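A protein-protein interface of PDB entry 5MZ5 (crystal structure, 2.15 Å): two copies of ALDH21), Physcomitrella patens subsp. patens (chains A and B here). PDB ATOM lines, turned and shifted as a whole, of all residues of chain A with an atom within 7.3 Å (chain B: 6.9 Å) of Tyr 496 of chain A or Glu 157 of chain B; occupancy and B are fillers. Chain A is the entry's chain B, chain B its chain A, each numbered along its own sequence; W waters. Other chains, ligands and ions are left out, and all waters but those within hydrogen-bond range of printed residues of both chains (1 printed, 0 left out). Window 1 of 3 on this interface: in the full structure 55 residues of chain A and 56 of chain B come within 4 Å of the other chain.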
ATOM      1  N   GLU A 150     -34.676 -21.488  37.837  1.00  0.00           N
ATOM      2  CA  GLU A 150     -33.221 -21.482  37.855  1.00  0.00           C
ATOM      3  C   GLU A 150     -32.660 -21.523  39.279  1.00  0.00           C
ATOM      4  O   GLU A 150     -31.571 -22.069  39.480  1.00  0.00           O
ATOM      5  CB  GLU A 150     -32.662 -20.281  37.079  1.00  0.00           C
ATOM      6  CG  GLU A 150     -32.847 -20.341  35.571  1.00  0.00           C
ATOM      7  CD  GLU A 150     -32.232 -21.513  34.819  1.00  0.00           C
ATOM      8  OE1 GLU A 150     -32.758 -21.847  33.735  1.00  0.00           O
ATOM      9  OE2 GLU A 150     -31.234 -22.096  35.298  1.00  0.00           O
ATOM     10  N   PRO A 201     -32.489 -12.515  38.939  1.00  0.00           N
ATOM     11  CA  PRO A 201     -31.265 -13.332  39.117  1.00  0.00           C
ATOM     12  C   PRO A 201     -30.596 -13.178  40.485  1.00  0.00           C
ATOM     13  O   PRO A 201     -30.067 -14.171  40.975  1.00  0.00           O
ATOM     14  CB  PRO A 201     -30.331 -12.838  38.002  1.00  0.00           C
ATOM     15  CG  PRO A 201     -31.217 -12.158  37.046  1.00  0.00           C
ATOM     16  CD  PRO A 201     -32.320 -11.566  37.811  1.00  0.00           C
ATOM     17  N   VAL A 283     -21.073  -5.351  34.926  1.00  0.00           N
ATOM     18  CA  VAL A 283     -21.976  -5.879  33.874  1.00  0.00           C
ATOM     19  C   VAL A 283     -22.637  -4.659  33.247  1.00  0.00           C
ATOM     20  O   VAL A 283     -23.182  -3.815  33.975  1.00  0.00           O
ATOM     21  CB  VAL A 283     -23.026  -6.933  34.367  1.00  0.00           C
ATOM     22  CG1 VAL A 283     -24.111  -7.196  33.299  1.00  0.00           C
ATOM     23  CG2 VAL A 283     -22.340  -8.235  34.756  1.00  0.00           C
ATOM     24  N   ASP A 477     -36.753 -13.703  27.074  1.00  0.00           N
ATOM     25  CA  ASP A 477     -36.226 -13.397  28.406  1.00  0.00           C
ATOM     26  C   ASP A 477     -35.270 -14.465  28.976  1.00  0.00           C
ATOM     27  O   ASP A 477     -34.606 -14.197  29.982  1.00  0.00           O
ATOM     28  CB  ASP A 477     -37.375 -13.053  29.372  1.00  0.00           C
ATOM     29  CG  ASP A 477     -38.098 -11.788  28.916  1.00  0.00           C
ATOM     30  OD1 ASP A 477     -37.526 -10.678  29.078  1.00  0.00           O
ATOM     31  OD2 ASP A 477     -39.178 -11.911  28.321  1.00  0.00           O
ATOM     32  N   SER A 478     -35.097 -15.597  28.275  1.00  0.00           N
ATOM     33  CA  SER A 478     -34.165 -16.653  28.688  1.00  0.00           C
ATOM     34  C   SER A 478     -32.875 -16.693  27.822  1.00  0.00           C
ATOM     35  O   SER A 478     -31.936 -17.406  28.170  1.00  0.00           O
ATOM     36  CB  SER A 478     -34.859 -18.019  28.683  1.00  0.00           C
ATOM     37  OG  SER A 478     -35.262 -18.350  27.367  1.00  0.00           O
ATOM     38  N   GLN A 479     -32.845 -15.948  26.698  1.00  0.00           N
ATOM     39  CA  GLN A 479     -31.717 -15.937  25.777  1.00  0.00           C
ATOM     40  C   GLN A 479     -30.525 -15.130  26.326  1.00  0.00           C
ATOM     41  O   GLN A 479     -30.767 -14.175  27.077  1.00  0.00           O
ATOM     42  CB  GLN A 479     -32.167 -15.377  24.411  1.00  0.00           C
ATOM     43  CG  GLN A 479     -32.048 -13.841  24.265  1.00  0.00           C
ATOM     44  CD  GLN A 479     -32.513 -13.311  22.938  1.00  0.00           C
ATOM     45  OE1 GLN A 479     -33.642 -13.531  22.509  1.00  0.00           O
ATOM     46  NE2 GLN A 479     -31.657 -12.583  22.268  1.00  0.00           N
ATOM     47  N   PRO A 480     -29.248 -15.462  25.974  1.00  0.00           N
ATOM     48  CA  PRO A 480     -28.121 -14.589  26.413  1.00  0.00           C
ATOM     49  C   PRO A 480     -28.220 -13.270  25.626  1.00  0.00           C
ATOM     50  O   PRO A 480     -28.170 -13.253  24.394  1.00  0.00           O
ATOM     51  CB  PRO A 480     -26.863 -15.395  26.068  1.00  0.00           C
ATOM     52  CG  PRO A 480     -27.289 -16.322  24.979  1.00  0.00           C
ATOM     53  CD  PRO A 480     -28.777 -16.563  25.098  1.00  0.00           C
ATOM     54  N   TYR A 481     -28.472 -12.187  26.341  1.00  0.00           N
ATOM     55  CA  TYR A 481     -28.696 -10.877  25.753  1.00  0.00           C
ATOM     56  C   TYR A 481     -27.600  -9.910  26.170  1.00  0.00           C
ATOM     57  O   TYR A 481     -27.319  -9.732  27.358  1.00  0.00           O
ATOM     58  CB  TYR A 481     -30.107 -10.365  26.136  1.00  0.00           C
ATOM     59  CG  TYR A 481     -30.363  -8.930  25.753  1.00  0.00           C
ATOM     60  CD1 TYR A 481     -30.789  -8.593  24.472  1.00  0.00           C
ATOM     61  CD2 TYR A 481     -30.157  -7.901  26.664  1.00  0.00           C
ATOM     62  CE1 TYR A 481     -31.017  -7.268  24.114  1.00  0.00           C
ATOM     63  CE2 TYR A 481     -30.345  -6.572  26.307  1.00  0.00           C
ATOM     64  CZ  TYR A 481     -30.788  -6.257  25.033  1.00  0.00           C
ATOM     65  OH  TYR A 481     -30.968  -4.934  24.688  1.00  0.00           O
ATOM     66  N   GLN A 490     -20.625  -8.540  28.956  1.00  0.00           N
ATOM     67  CA  GLN A 490     -21.373  -9.632  29.594  1.00  0.00           C
ATOM     68  C   GLN A 490     -22.787  -9.782  29.044  1.00  0.00           C
ATOM     69  O   GLN A 490     -23.180  -9.087  28.097  1.00  0.00           O
ATOM     70  CB  GLN A 490     -21.373  -9.566  31.152  1.00  0.00           C
ATOM     71  CG  GLN A 490     -20.002  -9.272  31.804  1.00  0.00           C
ATOM     72  CD  GLN A 490     -18.913 -10.253  31.398  1.00  0.00           C
ATOM     73  OE1 GLN A 490     -19.158 -11.453  31.190  1.00  0.00           O
ATOM     74  NE2 GLN A 490     -17.688  -9.751  31.252  1.00  0.00           N
ATOM     75  N   ARG A 491     -23.533 -10.751  29.596  1.00  0.00           N
ATOM     76  CA  ARG A 491     -24.874 -11.070  29.152  1.00  0.00           C
ATOM     77  C   ARG A 491     -25.883 -11.103  30.266  1.00  0.00           C
ATOM     78  O   ARG A 491     -25.593 -11.576  31.363  1.00  0.00           O
ATOM     79  CB  ARG A 491     -24.905 -12.443  28.425  1.00  0.00           C
ATOM     80  CG  ARG A 491     -24.013 -12.571  27.196  1.00  0.00           C
ATOM     81  CD  ARG A 491     -24.479 -11.698  26.041  1.00  0.00           C
ATOM     82  NE  ARG A 491     -23.581 -11.830  24.904  1.00  0.00           N
ATOM     83  CZ  ARG A 491     -22.488 -11.095  24.724  1.00  0.00           C
ATOM     84  NH1 ARG A 491     -22.181 -10.125  25.579  1.00  0.00           N
ATOM     85  NH2 ARG A 491     -21.706 -11.308  23.681  1.00  0.00           N
ATOM     86  N   GLU A 492     -27.096 -10.654  29.943  1.00  0.00           N
ATOM     87  CA  GLU A 492     -28.298 -10.783  30.749  1.00  0.00           C
ATOM     88  C   GLU A 492     -29.140 -11.862  30.078  1.00  0.00           C
ATOM     89  O   GLU A 492     -28.679 -12.491  29.126  1.00  0.00           O
ATOM     90  CB  GLU A 492     -29.024  -9.454  31.017  1.00  0.00           C
ATOM     91  CG  GLU A 492     -28.261  -8.644  32.045  1.00  0.00           C
ATOM     92  CD  GLU A 492     -28.950  -7.447  32.678  1.00  0.00           C
ATOM     93  OE1 GLU A 492     -30.112  -7.139  32.338  1.00  0.00           O
ATOM     94  OE2 GLU A 492     -28.315  -6.825  33.550  1.00  0.00           O
ATOM     95  N   GLY A 493     -30.296 -12.149  30.631  1.00  0.00           N
ATOM     96  CA  GLY A 493     -31.080 -13.335  30.326  1.00  0.00           C
ATOM     97  C   GLY A 493     -30.805 -14.061  31.624  1.00  0.00           C
ATOM     98  O   GLY A 493     -29.650 -14.077  32.079  1.00  0.00           O
ATOM     99  N   VAL A 494     -31.860 -14.509  32.307  1.00  0.00           N
ATOM    100  CA  VAL A 494     -31.820 -14.979  33.696  1.00  0.00           C
ATOM    101  C   VAL A 494     -30.594 -15.842  34.051  1.00  0.00           C
ATOM    102  O   VAL A 494     -29.833 -15.410  34.910  1.00  0.00           O
ATOM    103  CB  VAL A 494     -33.139 -15.634  34.164  1.00  0.00           C
ATOM    104  CG1 VAL A 494     -33.019 -16.125  35.608  1.00  0.00           C
ATOM    105  CG2 VAL A 494     -34.309 -14.650  34.027  1.00  0.00           C
ATOM    106  N   LYS A 495     -30.396 -17.020  33.419  1.00  0.00           N
ATOM    107  CA  LYS A 495     -29.288 -17.908  33.779  1.00  0.00           C
ATOM    108  C   LYS A 495     -27.887 -17.280  33.518  1.00  0.00           C
ATOM    109  O   LYS A 495     -26.974 -17.554  34.279  1.00  0.00           O
ATOM    110  CB  LYS A 495     -29.444 -19.313  33.143  1.00  0.00           C
ATOM    111  CG  LYS A 495     -29.140 -19.431  31.646  1.00  0.00           C
ATOM    112  CD  LYS A 495     -29.351 -20.876  31.187  1.00  0.00           C
ATOM    113  CE  LYS A 495     -28.815 -21.124  29.801  1.00  0.00           C
ATOM    114  NZ  LYS A 495     -28.688 -22.578  29.488  1.00  0.00           N
ATOM    115  N   TYR A 496     -27.744 -16.390  32.510  1.00  0.00           N
ATOM    116  CA  TYR A 496     -26.474 -15.709  32.214  1.00  0.00           C
ATOM    117  C   TYR A 496     -26.217 -14.592  33.188  1.00  0.00           C
ATOM    118  O   TYR A 496     -25.084 -14.414  33.631  1.00  0.00           O
ATOM    119  CB  TYR A 496     -26.428 -15.200  30.765  1.00  0.00           C
ATOM    120  CG  TYR A 496     -26.817 -16.277  29.777  1.00  0.00           C
ATOM    121  CD1 TYR A 496     -28.150 -16.472  29.418  1.00  0.00           C
ATOM    122  CD2 TYR A 496     -25.858 -17.127  29.228  1.00  0.00           C
ATOM    123  CE1 TYR A 496     -28.523 -17.506  28.564  1.00  0.00           C
ATOM    124  CE2 TYR A 496     -26.218 -18.155  28.351  1.00  0.00           C
ATOM    125  CZ  TYR A 496     -27.550 -18.329  28.012  1.00  0.00           C
ATOM    126  OH  TYR A 496     -27.910 -19.310  27.126  1.00  0.00           O
ATOM    127  N   ALA A 497     -27.275 -13.861  33.565  1.00  0.00           N
ATOM    128  CA  ALA A 497     -27.146 -12.806  34.567  1.00  0.00           C
ATOM    129  C   ALA A 497     -26.799 -13.481  35.922  1.00  0.00           C
ATOM    130  O   ALA A 497     -26.019 -12.930  36.691  1.00  0.00           O
ATOM    131  CB  ALA A 497     -28.448 -12.010  34.670  1.00  0.00           C
ATOM    132  N   MET A 498     -27.377 -14.667  36.208  1.00  0.00           N
ATOM    133  CA  MET A 498     -27.057 -15.407  37.452  1.00  0.00           C
ATOM    134  C   MET A 498     -25.546 -15.764  37.556  1.00  0.00           C
ATOM    135  O   MET A 498     -24.954 -15.601  38.623  1.00  0.00           O
ATOM    136  CB  MET A 498     -27.905 -16.659  37.570  1.00  0.00           C
ATOM    137  CG  MET A 498     -29.284 -16.377  38.041  1.00  0.00           C
ATOM    138  SD  MET A 498     -30.369 -17.795  37.898  1.00  0.00           S
ATOM    139  CE  MET A 498     -29.795 -18.800  39.238  1.00  0.00           C
ATOM    140  N   ASP A 499     -24.928 -16.165  36.429  1.00  0.00           N
ATOM    141  CA  ASP A 499     -23.511 -16.506  36.333  1.00  0.00           C
ATOM    142  C   ASP A 499     -22.599 -15.386  36.785  1.00  0.00           C
ATOM    143  O   ASP A 499     -21.626 -15.668  37.481  1.00  0.00           O
ATOM    144  CB  ASP A 499     -23.133 -16.951  34.911  1.00  0.00           C
ATOM    145  CG  ASP A 499     -23.016 -18.444  34.774  1.00  0.00           C
ATOM    146  OD1 ASP A 499     -22.259 -19.057  35.571  1.00  0.00           O
ATOM    147  OD2 ASP A 499     -23.678 -19.011  33.876  1.00  0.00           O
ATOM    148  N   ASP A 500     -22.919 -14.123  36.430  1.00  0.00           N
ATOM    149  CA  ASP A 500     -22.127 -12.968  36.847  1.00  0.00           C
ATOM    150  C   ASP A 500     -22.288 -12.648  38.333  1.00  0.00           C
ATOM    151  O   ASP A 500     -21.436 -11.971  38.899  1.00  0.00           O
ATOM    152  CB  ASP A 500     -22.426 -11.745  35.975  1.00  0.00           C
ATOM    153  CG  ASP A 500     -22.015 -11.906  34.521  1.00  0.00           C
ATOM    154  OD1 ASP A 500     -20.884 -12.356  34.270  1.00  0.00           O
ATOM    155  OD2 ASP A 500     -22.828 -11.582  33.641  1.00  0.00           O
ATOM    156  N   MET A 501     -23.369 -13.134  38.963  1.00  0.00           N
ATOM    157  CA  MET A 501     -23.644 -12.947  40.394  1.00  0.00           C
ATOM    158  C   MET A 501     -23.148 -14.142  41.224  1.00  0.00           C
ATOM    159  O   MET A 501     -23.464 -14.256  42.412  1.00  0.00           O
ATOM    160  CB  MET A 501     -25.151 -12.721  40.599  1.00  0.00           C
ATOM    161  CG  MET A 501     -25.580 -11.365  40.155  1.00  0.00           C
ATOM    162  SD  MET A 501     -27.352 -11.184  40.087  1.00  0.00           S
ATOM    163  CE  MET A 501     -27.481  -9.652  39.110  1.00  0.00           C
ATOM    164  N   TYR B 155     -17.756 -26.370  22.989  1.00  0.00           N
ATOM    165  CA  TYR B 155     -19.151 -26.705  22.722  1.00  0.00           C
ATOM    166  C   TYR B 155     -20.061 -25.507  22.827  1.00  0.00           C
ATOM    167  O   TYR B 155     -19.777 -24.538  23.540  1.00  0.00           O
ATOM    168  CB  TYR B 155     -19.643 -27.821  23.678  1.00  0.00           C
ATOM    169  CG  TYR B 155     -18.863 -29.110  23.562  1.00  0.00           C
ATOM    170  CD1 TYR B 155     -18.667 -29.721  22.327  1.00  0.00           C
ATOM    171  CD2 TYR B 155     -18.309 -29.719  24.687  1.00  0.00           C
ATOM    172  CE1 TYR B 155     -17.955 -30.914  22.213  1.00  0.00           C
ATOM    173  CE2 TYR B 155     -17.610 -30.925  24.587  1.00  0.00           C
ATOM    174  CZ  TYR B 155     -17.435 -31.518  23.347  1.00  0.00           C
ATOM    175  OH  TYR B 155     -16.720 -32.685  23.222  1.00  0.00           O
ATOM    176  N   GLY B 156     -21.146 -25.581  22.091  1.00  0.00           N
ATOM    177  CA  GLY B 156     -22.192 -24.583  22.146  1.00  0.00           C
ATOM    178  C   GLY B 156     -23.467 -25.275  22.585  1.00  0.00           C
ATOM    179  O   GLY B 156     -23.467 -26.477  22.864  1.00  0.00           O
ATOM    180  N   GLU B 157     -24.557 -24.536  22.639  1.00  0.00           N
ATOM    181  CA  GLU B 157     -25.827 -25.135  23.042  1.00  0.00           C
ATOM    182  C   GLU B 157     -26.874 -24.970  21.968  1.00  0.00           C
ATOM    183  O   GLU B 157     -26.896 -23.974  21.256  1.00  0.00           O
ATOM    184  CB  GLU B 157     -26.406 -24.429  24.287  1.00  0.00           C
ATOM    185  CG  GLU B 157     -25.541 -24.251  25.523  1.00  0.00           C
ATOM    186  CD  GLU B 157     -26.371 -23.587  26.609  1.00  0.00           C
ATOM    187  OE1 GLU B 157     -26.399 -22.332  26.663  1.00  0.00           O
ATOM    188  OE2 GLU B 157     -27.091 -24.325  27.323  1.00  0.00           O
ATOM    189  N   HIS B 158     -27.783 -25.915  21.919  1.00  0.00           N
ATOM    190  CA  HIS B 158     -29.011 -25.813  21.180  1.00  0.00           C
ATOM    191  C   HIS B 158     -30.064 -25.549  22.275  1.00  0.00           C
ATOM    192  O   HIS B 158     -30.216 -26.351  23.198  1.00  0.00           O
ATOM    193  CB  HIS B 158     -29.355 -27.048  20.360  1.00  0.00           C
ATOM    194  CG  HIS B 158     -30.574 -26.771  19.561  1.00  0.00           C
ATOM    195  ND1 HIS B 158     -31.837 -27.051  20.060  1.00  0.00           N
ATOM    196  CD2 HIS B 158     -30.701 -26.041  18.431  1.00  0.00           C
ATOM    197  CE1 HIS B 158     -32.684 -26.556  19.174  1.00  0.00           C
ATOM    198  NE2 HIS B 158     -32.041 -25.943  18.175  1.00  0.00           N
ATOM    199  N   ILE B 159     -30.699 -24.375  22.235  1.00  0.00           N
ATOM    200  CA  ILE B 159     -31.645 -24.003  23.283  1.00  0.00           C
ATOM    201  C   ILE B 159     -33.071 -23.838  22.760  1.00  0.00           C
ATOM    202  O   ILE B 159     -33.279 -23.180  21.734  1.00  0.00           O
ATOM    203  CB  ILE B 159     -31.184 -22.751  24.121  1.00  0.00           C
ATOM    204  CG1 ILE B 159     -31.066 -21.457  23.265  1.00  0.00           C
ATOM    205  CG2 ILE B 159     -29.883 -23.034  24.900  1.00  0.00           C
ATOM    206  CD1 ILE B 159     -30.894 -20.103  24.097  1.00  0.00           C
ATOM    207  N   GLY B 172     -32.865 -21.501  19.542  1.00  0.00           N
ATOM    208  CA  GLY B 172     -31.599 -20.796  19.454  1.00  0.00           C
ATOM    209  C   GLY B 172     -30.398 -21.697  19.428  1.00  0.00           C
ATOM    210  O   GLY B 172     -30.425 -22.808  19.971  1.00  0.00           O
ATOM    211  N   ILE B 173     -29.354 -21.237  18.755  1.00  0.00           N
ATOM    212  CA  ILE B 173     -28.045 -21.887  18.730  1.00  0.00           C
ATOM    213  C   ILE B 173     -27.108 -20.884  19.394  1.00  0.00           C
ATOM    214  O   ILE B 173     -26.970 -19.761  18.914  1.00  0.00           O
ATOM    215  CB  ILE B 173     -27.556 -22.304  17.313  1.00  0.00           C
ATOM    216  CG1 ILE B 173     -28.485 -23.385  16.704  1.00  0.00           C
ATOM    217  CG2 ILE B 173     -26.072 -22.784  17.376  1.00  0.00           C
ATOM    218  CD1 ILE B 173     -28.403 -23.500  15.197  1.00  0.00           C
ATOM    219  N   VAL B 174     -26.515 -21.283  20.521  1.00  0.00           N
ATOM    220  CA  VAL B 174     -25.578 -20.459  21.280  1.00  0.00           C
ATOM    221  C   VAL B 174     -24.178 -20.977  20.989  1.00  0.00           C
ATOM    222  O   VAL B 174     -23.899 -22.144  21.229  1.00  0.00           O
ATOM    223  CB  VAL B 174     -25.890 -20.453  22.800  1.00  0.00           C
ATOM    224  CG1 VAL B 174     -24.953 -19.507  23.540  1.00  0.00           C
ATOM    225  CG2 VAL B 174     -27.344 -20.077  23.060  1.00  0.00           C
ATOM    226  N   LYS B 175     -23.315 -20.118  20.449  1.00  0.00           N
ATOM    227  CA  LYS B 175     -21.953 -20.478  20.076  1.00  0.00           C
ATOM    228  C   LYS B 175     -20.996 -19.433  20.648  1.00  0.00           C
ATOM    229  O   LYS B 175     -21.392 -18.301  20.899  1.00  0.00           O
ATOM    230  CB  LYS B 175     -21.869 -20.547  18.532  1.00  0.00           C
ATOM    231  CG  LYS B 175     -20.726 -21.337  17.955  1.00  0.00           C
ATOM    232  CD  LYS B 175     -21.058 -21.757  16.539  1.00  0.00           C
ATOM    233  CE  LYS B 175     -20.039 -21.286  15.536  1.00  0.00           C
ATOM    234  NZ  LYS B 175     -20.298 -21.877  14.196  1.00  0.00           N
ATOM    235  N   THR B 504     -20.032 -14.862  23.773  1.00  0.00           N
ATOM    236  CA  THR B 504     -21.263 -15.593  23.491  1.00  0.00           C
ATOM    237  C   THR B 504     -22.046 -14.895  22.368  1.00  0.00           C
ATOM    238  O   THR B 504     -22.208 -13.677  22.402  1.00  0.00           O
ATOM    239  CB  THR B 504     -22.101 -15.715  24.779  1.00  0.00           C
ATOM    240  OG1 THR B 504     -21.352 -16.487  25.714  1.00  0.00           O
ATOM    241  CG2 THR B 504     -23.457 -16.396  24.539  1.00  0.00           C
ATOM    242  N   VAL B 506     -25.776 -15.662  20.119  1.00  0.00           N
ATOM    243  CA  VAL B 506     -26.956 -16.528  19.911  1.00  0.00           C
ATOM    244  C   VAL B 506     -27.580 -16.275  18.527  1.00  0.00           C
ATOM    245  O   VAL B 506     -27.693 -15.136  18.097  1.00  0.00           O
ATOM    246  CB  VAL B 506     -27.991 -16.435  21.076  1.00  0.00           C
ATOM    247  CG1 VAL B 506     -28.520 -14.993  21.270  1.00  0.00           C
ATOM    248  CG2 VAL B 506     -29.150 -17.444  20.904  1.00  0.00           C
HETATM  249  O   HOH W   1     -25.547 -13.482  23.409  1.00  0.00           O
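Water W1 lies within hydrogen-bond range of O of Pro 480 of chain A, NE of Arg 491 of chain A and O of Thr 504 of chain B.
The backbone carbonyl oxygen (O) of Glu 157 of chain B sits at hydrogen-bond distance from the backbone NH (N) of Val 174 of chain B.
Printed residues of chain B within 4 Å of Arg 491 of chain A: Thr 504.
Printed residues of chain B within 4 Å of Lys 495 of chain A: Glu 157 (3.2 Å).
Ile 159 of chain B touches none of the printed residues of chain A.
Printed residues of chain A within 4 Å of Val 506 of chain B: Pro 480.
The side-chain hydroxyl of Tyr 496 of chain A sits at hydrogen-bond distance from the side-chain carboxylate of Glu 157 of chain B, 3.4 Å away.
The backbone carbonyl oxygen (O) of Thr 504 of chain B sits at hydrogen-bond distance from the guanidinium group (NH2) of Arg 491 of chain A (2.7 Å).
The side-chain carboxylate (OE2) of Glu 157 of chain B lies within salt-bridge range of the side-chain amino group (NZ) of Lys 495 of chain A, 3.2 Å away.
Of the 20 printed residues of chain A, 4 touch a printed residue of chain B.
Of the 11 printed residues of chain B, 3 touch a printed residue of chain A.
Printed residues of chain B that touch a printed residue of chain A: Glu 157, Thr 504 and Val 506.
Hydrophobic or aromatic side chains of chain B within 4 Å of the printed part of chain A: Val 506.
Among the printed residues, 5 pairs touch across the chains.
Among the printed residues, Asp or Glu carboxylates within 4 Å of a Lys or Arg side-chain nitrogen of the other chain: Lys 495 of chain A with Glu 157 of chain B.
Pro 480 of chain A touches Thr 504 of chain B.
Pro 480 of chain A touches Val 506 of chain B (O to CG1, 3.6 Å).
No position is printed for both chains.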
